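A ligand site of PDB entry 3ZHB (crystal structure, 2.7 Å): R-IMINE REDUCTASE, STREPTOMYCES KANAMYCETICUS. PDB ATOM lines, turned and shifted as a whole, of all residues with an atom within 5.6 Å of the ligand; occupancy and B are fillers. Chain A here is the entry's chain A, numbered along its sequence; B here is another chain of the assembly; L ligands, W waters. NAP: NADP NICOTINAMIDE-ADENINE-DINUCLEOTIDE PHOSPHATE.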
ATOM      1  N   GLY A  26      -0.458  22.922 -23.908  1.00  0.00           N
ATOM      2  CA  GLY A  26      -0.094  24.326 -24.015  1.00  0.00           C
ATOM      3  C   GLY A  26       0.966  24.631 -22.988  1.00  0.00           C
ATOM      4  O   GLY A  26       0.744  24.365 -21.814  1.00  0.00           O
ATOM      5  N   LEU A  27       2.130  25.149 -23.418  1.00  0.00           N
ATOM      6  CA  LEU A  27       3.302  25.346 -22.527  1.00  0.00           C
ATOM      7  C   LEU A  27       3.962  26.699 -22.731  1.00  0.00           C
ATOM      8  O   LEU A  27       5.194  26.816 -22.790  1.00  0.00           O
ATOM      9  CB  LEU A  27       4.338  24.226 -22.726  1.00  0.00           C
ATOM     10  CG  LEU A  27       3.859  22.786 -22.484  1.00  0.00           C
ATOM     11  CD1 LEU A  27       4.970  21.788 -22.758  1.00  0.00           C
ATOM     12  CD2 LEU A  27       3.360  22.557 -21.065  1.00  0.00           C
ATOM     13  N   GLY A  28       3.138  27.712 -22.874  1.00  0.00           N
ATOM     14  CA  GLY A  28       3.569  29.111 -22.752  1.00  0.00           C
ATOM     15  C   GLY A  28       3.872  29.339 -21.299  1.00  0.00           C
ATOM     16  O   GLY A  28       3.963  28.375 -20.493  1.00  0.00           O
ATOM     17  N   LEU A  29       4.100  30.573 -20.951  1.00  0.00           N
ATOM     18  CA  LEU A  29       4.415  30.898 -19.544  1.00  0.00           C
ATOM     19  C   LEU A  29       3.426  30.242 -18.591  1.00  0.00           C
ATOM     20  O   LEU A  29       3.837  29.551 -17.660  1.00  0.00           O
ATOM     21  CB  LEU A  29       4.402  32.409 -19.306  1.00  0.00           C
ATOM     22  CG  LEU A  29       5.460  33.175 -20.114  1.00  0.00           C
ATOM     23  CD1 LEU A  29       5.395  34.666 -19.798  1.00  0.00           C
ATOM     24  CD2 LEU A  29       6.844  32.547 -19.850  1.00  0.00           C
ATOM     25  N   MET A  30       2.120  30.429 -18.851  1.00  0.00           N
ATOM     26  CA  MET A  30       1.114  29.924 -17.950  1.00  0.00           C
ATOM     27  C   MET A  30       0.971  28.407 -17.996  1.00  0.00           C
ATOM     28  O   MET A  30       0.781  27.769 -16.975  1.00  0.00           O
ATOM     29  CB  MET A  30      -0.215  30.585 -18.221  1.00  0.00           C
ATOM     30  CG  MET A  30      -1.281  30.190 -17.211  1.00  0.00           C
ATOM     31  SD  MET A  30      -0.881  30.664 -15.530  1.00  0.00           S
ATOM     32  CE  MET A  30      -1.204  32.426 -15.670  1.00  0.00           C
ATOM     33  N   GLY A  31       1.063  27.842 -19.184  1.00  0.00           N
ATOM     34  CA  GLY A  31       0.993  26.389 -19.307  1.00  0.00           C
ATOM     35  C   GLY A  31       2.053  25.651 -18.509  1.00  0.00           C
ATOM     36  O   GLY A  31       1.761  24.643 -17.854  1.00  0.00           O
ATOM     37  N   TRP A  48       2.164  18.363 -23.493  1.00  0.00           N
ATOM     38  CA  TRP A  48       2.301  18.566 -24.940  1.00  0.00           C
ATOM     39  C   TRP A  48       2.269  20.038 -25.296  1.00  0.00           C
ATOM     40  O   TRP A  48       1.515  20.808 -24.686  1.00  0.00           O
ATOM     41  CB  TRP A  48       1.206  17.836 -25.718  1.00  0.00           C
ATOM     42  CG  TRP A  48       1.352  17.944 -27.204  1.00  0.00           C
ATOM     43  CD1 TRP A  48       1.878  17.003 -28.027  1.00  0.00           C
ATOM     44  CD2 TRP A  48       0.917  19.017 -28.052  1.00  0.00           C
ATOM     45  NE1 TRP A  48       1.810  17.420 -29.325  1.00  0.00           N
ATOM     46  CE2 TRP A  48       1.233  18.662 -29.361  1.00  0.00           C
ATOM     47  CE3 TRP A  48       0.270  20.245 -27.809  1.00  0.00           C
ATOM     48  CZ2 TRP A  48       0.962  19.490 -30.441  1.00  0.00           C
ATOM     49  CZ3 TRP A  48       0.003  21.080 -28.896  1.00  0.00           C
ATOM     50  CH2 TRP A  48       0.342  20.693 -30.194  1.00  0.00           C
ATOM     51  N   ASN A  49       3.087  20.450 -26.271  1.00  0.00           N
ATOM     52  CA  ASN A  49       3.048  21.815 -26.812  1.00  0.00           C
ATOM     53  C   ASN A  49       3.392  21.756 -28.295  1.00  0.00           C
ATOM     54  O   ASN A  49       4.086  20.845 -28.721  1.00  0.00           O
ATOM     55  CB  ASN A  49       3.994  22.763 -26.101  1.00  0.00           C
ATOM     56  CG  ASN A  49       3.739  24.231 -26.447  1.00  0.00           C
ATOM     57  OD1 ASN A  49       2.671  24.777 -26.173  1.00  0.00           O
ATOM     58  ND2 ASN A  49       4.740  24.894 -27.021  1.00  0.00           N
ATOM     59  N   ARG A  50       2.820  22.659 -29.065  1.00  0.00           N
ATOM     60  CA  ARG A  50       3.057  22.721 -30.509  1.00  0.00           C
ATOM     61  C   ARG A  50       4.558  22.730 -30.821  1.00  0.00           C
ATOM     62  O   ARG A  50       5.078  21.777 -31.422  1.00  0.00           O
ATOM     63  CB  ARG A  50       2.422  23.975 -31.088  1.00  0.00           C
ATOM     64  CG  ARG A  50       2.725  24.156 -32.550  1.00  0.00           C
ATOM     65  CD  ARG A  50       2.036  25.362 -33.121  1.00  0.00           C
ATOM     66  NE  ARG A  50       2.388  26.611 -32.445  1.00  0.00           N
ATOM     67  CZ  ARG A  50       1.903  27.807 -32.834  1.00  0.00           C
ATOM     68  NH1 ARG A  50       1.050  27.910 -33.876  1.00  0.00           N
ATOM     69  NH2 ARG A  50       2.229  28.923 -32.182  1.00  0.00           N
ATOM     70  N   THR A  51       5.199  23.748 -30.324  1.00  0.00           N
ATOM     71  CA  THR A  51       6.625  23.850 -30.249  1.00  0.00           C
ATOM     72  C   THR A  51       7.121  22.878 -29.168  1.00  0.00           C
ATOM     73  O   THR A  51       7.390  23.311 -28.077  1.00  0.00           O
ATOM     74  CB  THR A  51       6.959  25.297 -29.844  1.00  0.00           C
ATOM     75  OG1 THR A  51       6.736  26.170 -30.957  1.00  0.00           O
ATOM     76  CG2 THR A  51       8.353  25.445 -29.409  1.00  0.00           C
ATOM     77  N   LYS A  54       9.581  22.712 -25.317  1.00  0.00           N
ATOM     78  CA  LYS A  54       9.516  24.075 -24.813  1.00  0.00           C
ATOM     79  C   LYS A  54       9.317  24.086 -23.288  1.00  0.00           C
ATOM     80  O   LYS A  54       8.414  24.757 -22.783  1.00  0.00           O
ATOM     81  CB  LYS A  54       8.393  24.852 -25.487  1.00  0.00           C
ATOM     82  CG  LYS A  54       8.326  26.326 -25.107  1.00  0.00           C
ATOM     83  CD  LYS A  54       7.935  27.186 -26.285  1.00  0.00           C
ATOM     84  CE  LYS A  54       7.401  28.540 -25.828  1.00  0.00           C
ATOM     85  NZ  LYS A  54       6.332  29.056 -26.729  1.00  0.00           N
ATOM     86  N   CYS A  82      -4.365  25.174 -21.858  1.00  0.00           N
ATOM     87  CA  CYS A  82      -4.051  26.561 -21.679  1.00  0.00           C
ATOM     88  C   CYS A  82      -3.189  27.062 -22.841  1.00  0.00           C
ATOM     89  O   CYS A  82      -1.986  26.897 -22.832  1.00  0.00           O
ATOM     90  CB  CYS A  82      -3.355  26.799 -20.351  1.00  0.00           C
ATOM     91  SG  CYS A  82      -3.279  28.563 -19.984  1.00  0.00           S
ATOM     92  N   VAL A  83      -3.836  27.687 -23.812  1.00  0.00           N
ATOM     93  CA  VAL A  83      -3.186  28.173 -25.021  1.00  0.00           C
ATOM     94  C   VAL A  83      -3.646  29.584 -25.217  1.00  0.00           C
ATOM     95  O   VAL A  83      -4.329  30.131 -24.346  1.00  0.00           O
ATOM     96  CB  VAL A  83      -3.502  27.329 -26.231  1.00  0.00           C
ATOM     97  CG1 VAL A  83      -2.917  25.927 -26.056  1.00  0.00           C
ATOM     98  CG2 VAL A  83      -5.000  27.285 -26.493  1.00  0.00           C
ATOM     99  N   SER A  84      -3.270  30.212 -26.309  1.00  0.00           N
ATOM    100  CA  SER A  84      -3.392  31.694 -26.338  1.00  0.00           C
ATOM    101  C   SER A  84      -4.827  32.163 -26.381  1.00  0.00           C
ATOM    102  O   SER A  84      -5.191  33.033 -25.652  1.00  0.00           O
ATOM    103  CB  SER A  84      -2.606  32.279 -27.520  1.00  0.00           C
ATOM    104  OG  SER A  84      -3.075  31.659 -28.704  1.00  0.00           O
ATOM    105  N   ASP A  85      -5.631  31.571 -27.268  1.00  0.00           N
ATOM    106  CA  ASP A  85      -7.046  31.913 -27.417  1.00  0.00           C
ATOM    107  C   ASP A  85      -7.880  30.714 -27.907  1.00  0.00           C
ATOM    108  O   ASP A  85      -7.360  29.625 -28.138  1.00  0.00           O
ATOM    109  CB  ASP A  85      -7.217  33.119 -28.312  1.00  0.00           C
ATOM    110  CG  ASP A  85      -6.617  32.925 -29.710  1.00  0.00           C
ATOM    111  OD1 ASP A  85      -6.540  31.781 -30.250  1.00  0.00           O
ATOM    112  OD2 ASP A  85      -6.234  33.946 -30.303  1.00  0.00           O
ATOM    113  N   ALA A  88      -6.928  28.918 -31.152  1.00  0.00           N
ATOM    114  CA  ALA A  88      -5.980  27.857 -30.928  1.00  0.00           C
ATOM    115  C   ALA A  88      -6.656  26.615 -30.378  1.00  0.00           C
ATOM    116  O   ALA A  88      -6.285  25.495 -30.752  1.00  0.00           O
ATOM    117  CB  ALA A  88      -4.859  28.317 -29.997  1.00  0.00           C
ATOM    118  N   ALA A  91      -8.182  24.789 -33.026  1.00  0.00           N
ATOM    119  CA  ALA A  91      -7.174  24.174 -33.872  1.00  0.00           C
ATOM    120  C   ALA A  91      -6.651  22.823 -33.317  1.00  0.00           C
ATOM    121  O   ALA A  91      -6.406  21.904 -34.086  1.00  0.00           O
ATOM    122  CB  ALA A  91      -6.035  25.124 -34.106  1.00  0.00           C
ATOM    123  N   LEU A  92      -6.519  22.719 -32.009  1.00  0.00           N
ATOM    124  CA  LEU A  92      -5.958  21.531 -31.419  1.00  0.00           C
ATOM    125  C   LEU A  92      -6.982  20.497 -31.103  1.00  0.00           C
ATOM    126  O   LEU A  92      -6.650  19.336 -31.019  1.00  0.00           O
ATOM    127  CB  LEU A  92      -5.259  21.888 -30.116  1.00  0.00           C
ATOM    128  CG  LEU A  92      -4.137  22.898 -30.204  1.00  0.00           C
ATOM    129  CD1 LEU A  92      -3.553  23.166 -28.832  1.00  0.00           C
ATOM    130  CD2 LEU A  92      -3.097  22.347 -31.173  1.00  0.00           C
ATOM    131  N   LEU A 109      -8.540  26.436 -19.425  1.00  0.00           N
ATOM    132  CA  LEU A 109      -8.170  27.641 -18.686  1.00  0.00           C
ATOM    133  C   LEU A 109      -7.648  28.743 -19.600  1.00  0.00           C
ATOM    134  O   LEU A 109      -7.008  29.707 -19.170  1.00  0.00           O
ATOM    135  CB  LEU A 109      -7.115  27.291 -17.646  1.00  0.00           C
ATOM    136  CG  LEU A 109      -7.592  26.273 -16.615  1.00  0.00           C
ATOM    137  CD1 LEU A 109      -6.431  26.018 -15.680  1.00  0.00           C
ATOM    138  CD2 LEU A 109      -8.819  26.728 -15.859  1.00  0.00           C
ATOM    139  N   THR A 110      -7.902  28.589 -20.894  1.00  0.00           N
ATOM    140  CA  THR A 110      -7.696  29.674 -21.844  1.00  0.00           C
ATOM    141  C   THR A 110      -8.682  30.794 -21.610  1.00  0.00           C
ATOM    142  O   THR A 110      -9.886  30.576 -21.309  1.00  0.00           O
ATOM    143  CB  THR A 110      -7.861  29.140 -23.278  1.00  0.00           C
ATOM    144  OG1 THR A 110      -7.005  28.027 -23.457  1.00  0.00           O
ATOM    145  CG2 THR A 110      -7.537  30.189 -24.293  1.00  0.00           C
ATOM    146  N   SER A 111      -8.182  31.987 -21.758  1.00  0.00           N
ATOM    147  CA  SER A 111      -9.007  33.201 -21.692  1.00  0.00           C
ATOM    148  C   SER A 111      -9.857  33.391 -22.920  1.00  0.00           C
ATOM    149  O   SER A 111      -9.373  33.208 -24.023  1.00  0.00           O
ATOM    150  CB  SER A 111      -8.134  34.464 -21.528  1.00  0.00           C
ATOM    151  OG  SER A 111      -7.186  34.349 -20.469  1.00  0.00           O
ATOM    152  N   ILE A 136      -7.686  32.160 -15.452  1.00  0.00           N
ATOM    153  CA  ILE A 136      -6.610  32.407 -14.448  1.00  0.00           C
ATOM    154  C   ILE A 136      -6.506  33.909 -14.190  1.00  0.00           C
ATOM    155  O   ILE A 136      -6.369  34.663 -15.125  1.00  0.00           O
ATOM    156  CB  ILE A 136      -5.224  32.035 -14.958  1.00  0.00           C
ATOM    157  CG1 ILE A 136      -5.160  30.723 -15.728  1.00  0.00           C
ATOM    158  CG2 ILE A 136      -4.251  32.048 -13.828  1.00  0.00           C
ATOM    159  CD1 ILE A 136      -5.505  29.520 -14.950  1.00  0.00           C
ATOM    160  N   LEU A 137      -6.555  34.347 -12.937  1.00  0.00           N
ATOM    161  CA  LEU A 137      -6.491  35.792 -12.638  1.00  0.00           C
ATOM    162  C   LEU A 137      -5.244  36.084 -11.804  1.00  0.00           C
ATOM    163  O   LEU A 137      -5.300  36.671 -10.736  1.00  0.00           O
ATOM    164  CB  LEU A 137      -7.766  36.232 -11.916  1.00  0.00           C
ATOM    165  CG  LEU A 137      -9.028  36.523 -12.744  1.00  0.00           C
ATOM    166  CD1 LEU A 137      -9.448  35.309 -13.546  1.00  0.00           C
ATOM    167  CD2 LEU A 137     -10.142  36.950 -11.822  1.00  0.00           C
ATOM    168  N   ALA A 138      -4.109  35.621 -12.273  1.00  0.00           N
ATOM    169  CA  ALA A 138      -2.885  35.770 -11.525  1.00  0.00           C
ATOM    170  C   ALA A 138      -1.826  35.427 -12.505  1.00  0.00           C
ATOM    171  O   ALA A 138      -2.128  34.839 -13.532  1.00  0.00           O
ATOM    172  CB  ALA A 138      -2.835  34.817 -10.339  1.00  0.00           C
ATOM    173  N   GLY A 139      -0.588  35.771 -12.199  1.00  0.00           N
ATOM    174  CA  GLY A 139       0.518  35.501 -13.109  1.00  0.00           C
ATOM    175  C   GLY A 139       1.090  34.110 -12.860  1.00  0.00           C
ATOM    176  O   GLY A 139       0.737  33.485 -11.870  1.00  0.00           O
ATOM    177  N   PRO A 140       1.963  33.643 -13.761  1.00  0.00           N
ATOM    178  CA  PRO A 140       2.487  32.285 -13.677  1.00  0.00           C
ATOM    179  C   PRO A 140       3.153  32.029 -12.367  1.00  0.00           C
ATOM    180  O   PRO A 140       3.004  30.940 -11.813  1.00  0.00           O
ATOM    181  CB  PRO A 140       3.505  32.224 -14.826  1.00  0.00           C
ATOM    182  CG  PRO A 140       2.993  33.223 -15.817  1.00  0.00           C
ATOM    183  CD  PRO A 140       2.351  34.316 -15.012  1.00  0.00           C
ATOM    184  N   ASP B 249       6.935  41.006 -19.053  1.00  0.00           N
ATOM    185  CA  ASP B 249       6.019  40.002 -19.606  1.00  0.00           C
ATOM    186  C   ASP B 249       4.537  40.449 -19.607  1.00  0.00           C
ATOM    187  O   ASP B 249       3.623  39.599 -19.523  1.00  0.00           O
ATOM    188  CB  ASP B 249       6.172  38.672 -18.821  1.00  0.00           C
ATOM    189  CG  ASP B 249       7.481  37.937 -19.136  1.00  0.00           C
ATOM    190  OD1 ASP B 249       7.881  37.905 -20.323  1.00  0.00           O
ATOM    191  OD2 ASP B 249       8.117  37.371 -18.223  1.00  0.00           O
HETATM  192  PA  NAP L   1       1.834  32.400 -24.340  1.00  0.00           P
HETATM  193  O1A NAP L   1       3.216  32.601 -23.641  1.00  0.00           O
HETATM  194  O2A NAP L   1       1.416  33.100 -25.627  1.00  0.00           O
HETATM  195  O5B NAP L   1       1.599  30.837 -24.592  1.00  0.00           O
HETATM  196  C5B NAP L   1       0.571  30.698 -25.533  1.00  0.00           C
HETATM  197  C4B NAP L   1       0.424  29.255 -25.905  1.00  0.00           C
HETATM  198  O4B NAP L   1      -0.314  29.393 -27.100  1.00  0.00           O
HETATM  199  C3B NAP L   1       1.707  28.523 -26.253  1.00  0.00           C
HETATM  200  O3B NAP L   1       1.808  27.233 -25.628  1.00  0.00           O
HETATM  201  C2B NAP L   1       1.588  28.372 -27.759  1.00  0.00           C
HETATM  202  O2B NAP L   1       2.301  27.248 -28.291  1.00  0.00           O
HETATM  203  C1B NAP L   1       0.085  28.296 -27.874  1.00  0.00           C
HETATM  204  N9A NAP L   1      -0.518  28.537 -29.176  1.00  0.00           N
HETATM  205  C8A NAP L   1      -0.875  29.726 -29.707  1.00  0.00           C
HETATM  206  N7A NAP L   1      -1.446  29.548 -30.943  1.00  0.00           N
HETATM  207  C5A NAP L   1      -1.443  28.204 -31.123  1.00  0.00           C
HETATM  208  C6A NAP L   1      -1.879  27.319 -32.176  1.00  0.00           C
HETATM  209  N6A NAP L   1      -2.427  27.956 -33.200  1.00  0.00           N
HETATM  210  N1A NAP L   1      -1.751  25.983 -32.104  1.00  0.00           N
HETATM  211  C2A NAP L   1      -1.175  25.455 -30.979  1.00  0.00           C
HETATM  212  N3A NAP L   1      -0.719  26.192 -29.938  1.00  0.00           N
HETATM  213  C4A NAP L   1      -0.849  27.538 -29.964  1.00  0.00           C
HETATM  214  O3  NAP L   1       0.571  32.815 -23.399  1.00  0.00           O
HETATM  215  PN  NAP L   1       0.358  32.261 -21.897  1.00  0.00           P
HETATM  216  O1N NAP L   1       0.733  33.420 -21.021  1.00  0.00           O
HETATM  217  O2N NAP L   1       0.889  30.855 -21.524  1.00  0.00           O
HETATM  218  O5D NAP L   1      -1.192  32.200 -22.234  1.00  0.00           O
HETATM  219  C5D NAP L   1      -2.071  31.065 -22.110  1.00  0.00           C
HETATM  220  C4D NAP L   1      -3.403  31.548 -21.513  1.00  0.00           C
HETATM  221  O4D NAP L   1      -3.197  31.946 -20.147  1.00  0.00           O
HETATM  222  C3D NAP L   1      -3.897  32.780 -22.261  1.00  0.00           C
HETATM  223  O3D NAP L   1      -5.274  32.680 -22.558  1.00  0.00           O
HETATM  224  C2D NAP L   1      -3.624  33.906 -21.324  1.00  0.00           C
HETATM  225  O2D NAP L   1      -4.551  34.962 -21.540  1.00  0.00           O
HETATM  226  C1D NAP L   1      -3.815  33.205 -20.002  1.00  0.00           C
HETATM  227  N1N NAP L   1      -3.295  33.980 -18.904  1.00  0.00           N
HETATM  228  C2N NAP L   1      -2.030  34.340 -18.905  1.00  0.00           C
HETATM  229  C3N NAP L   1      -1.519  35.109 -17.871  1.00  0.00           C
HETATM  230  C7N NAP L   1      -0.080  35.519 -17.878  1.00  0.00           C
HETATM  231  O7N NAP L   1       0.162  36.627 -17.433  1.00  0.00           O
HETATM  232  N7N NAP L   1       0.820  34.670 -18.395  1.00  0.00           N
HETATM  233  C4N NAP L   1      -2.351  35.507 -16.821  1.00  0.00           C
HETATM  234  C5N NAP L   1      -3.671  35.118 -16.860  1.00  0.00           C
HETATM  235  C6N NAP L   1      -4.121  34.338 -17.915  1.00  0.00           C
HETATM  236  P2B NAP L   1       3.703  27.590 -29.079  1.00  0.00           P
HETATM  237  O1X NAP L   1       3.481  28.861 -29.897  1.00  0.00           O
HETATM  238  O2X NAP L   1       4.618  27.868 -27.944  1.00  0.00           O
HETATM  239  O3X NAP L   1       3.976  26.259 -29.777  1.00  0.00           O
HETATM  240  O   HOH W   1       0.369  28.045 -21.938  1.00  0.00           O
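O of Thr 51 is in hydrogen-bond range of ND2 of Asn 49. The backbone NH (N) of Val 83 sits at hydrogen-bond distance from the side-chain hydroxyl (OG1) of Thr 110 (3.2 Å). The side-chain amide oxygen (OD1) of Asn 49 sits at hydrogen-bond distance from the backbone NH (N) of Leu 27 (2.8 Å). The backbone NH (N) of Ala 88 sits at hydrogen-bond distance from the side-chain carboxylate (OD1) of Asp 85. N of Gly 26 lies within hydrogen-bond range of O of Trp 48, at 3.0 Å.
An oxygen (O3X) of the ligand lies within hydrogen-bond range of the side-chain hydroxyl of Thr 51, 3.0 Å away. An oxygen (O3D) of the ligand is in hydrogen-bond range of the backbone carbonyl oxygen (O) of Ser 84 (3.1 Å). The backbone carbonyl oxygen (O) of Val 83 lies within hydrogen-bond range of an oxygen (O3D) of the ligand (3.3 Å). NH2 of Arg 50 lies within salt-bridge range of O1X of the ligand, at 2.6 Å. O2D of the ligand lies within hydrogen-bond range of OG of Ser 111 (2.9 Å). N of Met 30 sits at hydrogen-bond distance from O2N of the ligand, 3.0 Å away. The side-chain amino group (NZ) of Lys 54 lies within salt-bridge range of an oxygen (O2X) of the ligand (2.4 Å). N of Ser 84 lies within hydrogen-bond range of O4B of the ligand, 3.2 Å away. The side-chain hydroxyl (OG) of Ser 84 lies close to a nitrogen (N7A) of the ligand (3.5 Å). O3B of the ligand is in hydrogen-bond range of N of Gly 28, 3.1 Å away. The backbone NH (N) of Leu 29 lies within hydrogen-bond range of an oxygen (O2N) of the ligand (3.3 Å). OD1 of Asn 49 is in hydrogen-bond range of O3B of the ligand, 2.7 Å away. N of Leu 27 sits at hydrogen-bond distance from O3B of the ligand (3.1 Å). The backbone NH (N) of Ser 111 lies within hydrogen-bond range of an oxygen (O3D) of the ligand (3.1 Å). N of Thr 51 is in hydrogen-bond range of O3X of the ligand, at 2.8 Å. The side-chain sulfur (SG) of Cys 82 lies close to an oxygen (O4D) of the ligand (3.4 Å).
C of Gly 26 touches O3B of the ligand, 3.8 Å away. Gly 31 touches the ligand. Ala 88 touches the ligand. Leu 92 touches the ligand (CD2 to C2A, 3.7 Å). Thr 110 touches the ligand (CG2 to O3D, 3.8 Å). O of Ile 136 touches C5N of the ligand, 3.2 Å away. O of Ala 138 touches C4N of the ligand (3.4 Å). Pro 140 touches the ligand. Within 4 Å of the ligand: Gly 26, Leu 27, Gly 28, Leu 29, Met 30, Gly 31, Asn 49, Arg 50, Thr 51, Lys 54, Cys 82, Val 83, Ser 84, Ala 88, Leu 92, Thr 110, Ser 111, Ile 136, Ala 138 and Pro 140.
Water W1 lies within hydrogen-bond range of O of Cys 82 (2.8 Å), N of Gly 31 (2.8 Å), O2N of the ligand (2.9 Å) and N of Gly 28 (2.9 Å).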
